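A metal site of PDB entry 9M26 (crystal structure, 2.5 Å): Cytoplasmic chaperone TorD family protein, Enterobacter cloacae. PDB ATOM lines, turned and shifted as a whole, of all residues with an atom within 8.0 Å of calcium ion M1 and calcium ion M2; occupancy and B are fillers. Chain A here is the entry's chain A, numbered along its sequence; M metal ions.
Within 4 Å of calcium ion M2: Asp 181 and Glu 185.
Calcium ion M2 is bound by OE2 of Glu 185, 2.6 Å away.
OD1 of Asp 181 binds calcium ion M2.
Calcium ion M2 has two donor atoms within binding distance.
Within 4 Å of calcium ion M1: Asp 181, Glu 182 and Glu 185.
The nearest printed residue that does not touch calcium ion M1 is Ala 178 (6.1 Å).
Calcium ion M1 is bound by OD2 of Asp 181, at 2.4 Å.
OE2 of Glu 185 binds calcium ion M1.
Calcium ion M1 is bound by OE2 of Glu 182 (2.8 Å).
Calcium ion M1 has three donor atoms within binding distance.
Slightly farther from calcium ion M1 lies OE1 of Glu 185 (3.0 Å).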
ATOM      1  N   LYS A   3      25.001  13.549 -12.460  1.00  0.00           N
ATOM      2  CA  LYS A   3      24.551  13.152 -11.138  1.00  0.00           C
ATOM      3  C   LYS A   3      24.342  11.638 -11.107  1.00  0.00           C
ATOM      4  O   LYS A   3      23.920  11.039 -12.094  1.00  0.00           O
ATOM      5  CB  LYS A   3      23.263  13.895 -10.765  1.00  0.00           C
ATOM      6  CG  LYS A   3      23.351  14.790  -9.526  1.00  0.00           C
ATOM      7  CD  LYS A   3      22.125  15.723  -9.355  1.00  0.00           C
ATOM      8  CE  LYS A   3      20.976  15.088  -8.573  1.00  0.00           C
ATOM      9  NZ  LYS A   3      21.265  14.911  -7.120  1.00  0.00           N
ATOM     10  N   ALA A 177       7.862   8.615  -7.851  1.00  0.00           N
ATOM     11  CA  ALA A 177       7.773   9.728  -8.788  1.00  0.00           C
ATOM     12  C   ALA A 177       8.890  10.730  -8.558  1.00  0.00           C
ATOM     13  O   ALA A 177       9.404  11.326  -9.507  1.00  0.00           O
ATOM     14  CB  ALA A 177       6.402  10.401  -8.685  1.00  0.00           C
ATOM     15  N   ALA A 178       9.273  10.938  -7.297  1.00  0.00           N
ATOM     16  CA  ALA A 178      10.336  11.879  -6.983  1.00  0.00           C
ATOM     17  C   ALA A 178      11.690  11.341  -7.425  1.00  0.00           C
ATOM     18  O   ALA A 178      12.549  12.098  -7.902  1.00  0.00           O
ATOM     19  CB  ALA A 178      10.333  12.194  -5.494  1.00  0.00           C
ATOM     20  N   MET A 179      11.908  10.030  -7.270  1.00  0.00           N
ATOM     21  CA  MET A 179      13.150   9.434  -7.756  1.00  0.00           C
ATOM     22  C   MET A 179      13.229   9.489  -9.263  1.00  0.00           C
ATOM     23  O   MET A 179      14.283   9.839  -9.817  1.00  0.00           O
ATOM     24  CB  MET A 179      13.249   7.989  -7.294  1.00  0.00           C
ATOM     25  CG  MET A 179      13.564   7.801  -5.832  1.00  0.00           C
ATOM     26  SD  MET A 179      13.845   6.055  -5.474  1.00  0.00           S
ATOM     27  CE  MET A 179      12.277   5.330  -5.942  1.00  0.00           C
ATOM     28  N   TRP A 180      12.128   9.172  -9.935  1.00  0.00           N
ATOM     29  CA  TRP A 180      12.107   9.119 -11.398  1.00  0.00           C
ATOM     30  C   TRP A 180      12.416  10.479 -12.016  1.00  0.00           C
ATOM     31  O   TRP A 180      13.129  10.558 -13.026  1.00  0.00           O
ATOM     32  CB  TRP A 180      10.768   8.589 -11.894  1.00  0.00           C
ATOM     33  CG  TRP A 180      10.737   8.417 -13.374  1.00  0.00           C
ATOM     34  CD1 TRP A 180       9.847   8.978 -14.260  1.00  0.00           C
ATOM     35  CD2 TRP A 180      11.673   7.680 -14.173  1.00  0.00           C
ATOM     36  NE1 TRP A 180      10.146   8.583 -15.547  1.00  0.00           N
ATOM     37  CE2 TRP A 180      11.270   7.790 -15.521  1.00  0.00           C
ATOM     38  CE3 TRP A 180      12.803   6.903 -13.874  1.00  0.00           C
ATOM     39  CZ2 TRP A 180      11.947   7.161 -16.558  1.00  0.00           C
ATOM     40  CZ3 TRP A 180      13.489   6.293 -14.917  1.00  0.00           C
ATOM     41  CH2 TRP A 180      13.053   6.424 -16.232  1.00  0.00           C
ATOM     42  N   ASP A 181      11.876  11.552 -11.428  1.00  0.00           N
ATOM     43  CA  ASP A 181      12.182  12.884 -11.942  1.00  0.00           C
ATOM     44  C   ASP A 181      13.673  13.167 -11.886  1.00  0.00           C
ATOM     45  O   ASP A 181      14.237  13.747 -12.827  1.00  0.00           O
ATOM     46  CB  ASP A 181      11.417  13.950 -11.146  1.00  0.00           C
ATOM     47  CG  ASP A 181      11.869  15.367 -11.477  1.00  0.00           C
ATOM     48  OD1 ASP A 181      11.429  15.937 -12.514  1.00  0.00           O
ATOM     49  OD2 ASP A 181      12.682  15.900 -10.689  1.00  0.00           O
ATOM     50  N   GLU A 182      14.346  12.728 -10.828  1.00  0.00           N
ATOM     51  CA  GLU A 182      15.777  13.020 -10.687  1.00  0.00           C
ATOM     52  C   GLU A 182      16.621  12.178 -11.653  1.00  0.00           C
ATOM     53  O   GLU A 182      17.609  12.661 -12.213  1.00  0.00           O
ATOM     54  CB  GLU A 182      16.190  12.769  -9.244  1.00  0.00           C
ATOM     55  CG  GLU A 182      17.090  13.839  -8.669  1.00  0.00           C
ATOM     56  CD  GLU A 182      16.462  15.227  -8.763  1.00  0.00           C
ATOM     57  OE1 GLU A 182      17.222  16.199  -8.951  1.00  0.00           O
ATOM     58  OE2 GLU A 182      15.218  15.346  -8.687  1.00  0.00           O
ATOM     59  N   LEU A 183      16.243  10.903 -11.842  1.00  0.00           N
ATOM     60  CA  LEU A 183      16.912  10.036 -12.813  1.00  0.00           C
ATOM     61  C   LEU A 183      16.701  10.523 -14.243  1.00  0.00           C
ATOM     62  O   LEU A 183      17.646  10.610 -15.031  1.00  0.00           O
ATOM     63  CB  LEU A 183      16.434   8.589 -12.650  1.00  0.00           C
ATOM     64  CG  LEU A 183      16.659   7.981 -11.259  1.00  0.00           C
ATOM     65  CD1 LEU A 183      15.735   6.793 -11.007  1.00  0.00           C
ATOM     66  CD2 LEU A 183      18.106   7.588 -11.072  1.00  0.00           C
ATOM     67  N   GLU A 184      15.443  10.817 -14.604  1.00  0.00           N
ATOM     68  CA  GLU A 184      15.154  11.264 -15.965  1.00  0.00           C
ATOM     69  C   GLU A 184      15.889  12.553 -16.286  1.00  0.00           C
ATOM     70  O   GLU A 184      16.299  12.748 -17.443  1.00  0.00           O
ATOM     71  CB  GLU A 184      13.664  11.463 -16.180  1.00  0.00           C
ATOM     72  CG  GLU A 184      12.957  10.260 -16.750  1.00  0.00           C
ATOM     73  CD  GLU A 184      13.508   9.798 -18.093  1.00  0.00           C
ATOM     74  OE1 GLU A 184      14.530   9.083 -18.109  1.00  0.00           O
ATOM     75  OE2 GLU A 184      12.906  10.124 -19.137  1.00  0.00           O
ATOM     76  N   GLU A 185      16.090  13.435 -15.294  1.00  0.00           N
ATOM     77  CA  GLU A 185      16.795  14.675 -15.569  1.00  0.00           C
ATOM     78  C   GLU A 185      18.242  14.405 -15.966  1.00  0.00           C
ATOM     79  O   GLU A 185      18.845  15.192 -16.696  1.00  0.00           O
ATOM     80  CB  GLU A 185      16.765  15.605 -14.352  1.00  0.00           C
ATOM     81  CG  GLU A 185      15.453  16.340 -14.125  1.00  0.00           C
ATOM     82  CD  GLU A 185      15.311  16.858 -12.698  1.00  0.00           C
ATOM     83  OE1 GLU A 185      16.087  16.443 -11.818  1.00  0.00           O
ATOM     84  OE2 GLU A 185      14.427  17.709 -12.459  1.00  0.00           O
ATOM     85  N   GLU A 186      18.788  13.274 -15.523  1.00  0.00           N
ATOM     86  CA  GLU A 186      20.119  12.854 -15.936  1.00  0.00           C
ATOM     87  C   GLU A 186      20.081  11.954 -17.160  1.00  0.00           C
ATOM     88  O   GLU A 186      21.013  11.993 -17.978  1.00  0.00           O
ATOM     89  CB  GLU A 186      20.819  12.116 -14.782  1.00  0.00           C
ATOM     90  CG  GLU A 186      20.965  12.959 -13.508  1.00  0.00           C
ATOM     91  CD  GLU A 186      21.502  14.362 -13.784  1.00  0.00           C
ATOM     92  OE1 GLU A 186      22.673  14.515 -14.194  1.00  0.00           O
ATOM     93  OE2 GLU A 186      20.733  15.327 -13.616  1.00  0.00           O
HETATM   94 CA    CA M   1      14.128  17.638  -9.922  1.00  0.00          CA
HETATM   95 CA    CA M   2      12.092  18.427 -13.294  1.00  0.00          CA
HETATM   96 CA    CA M   3      18.518  19.648 -16.918  1.00  0.00          CA
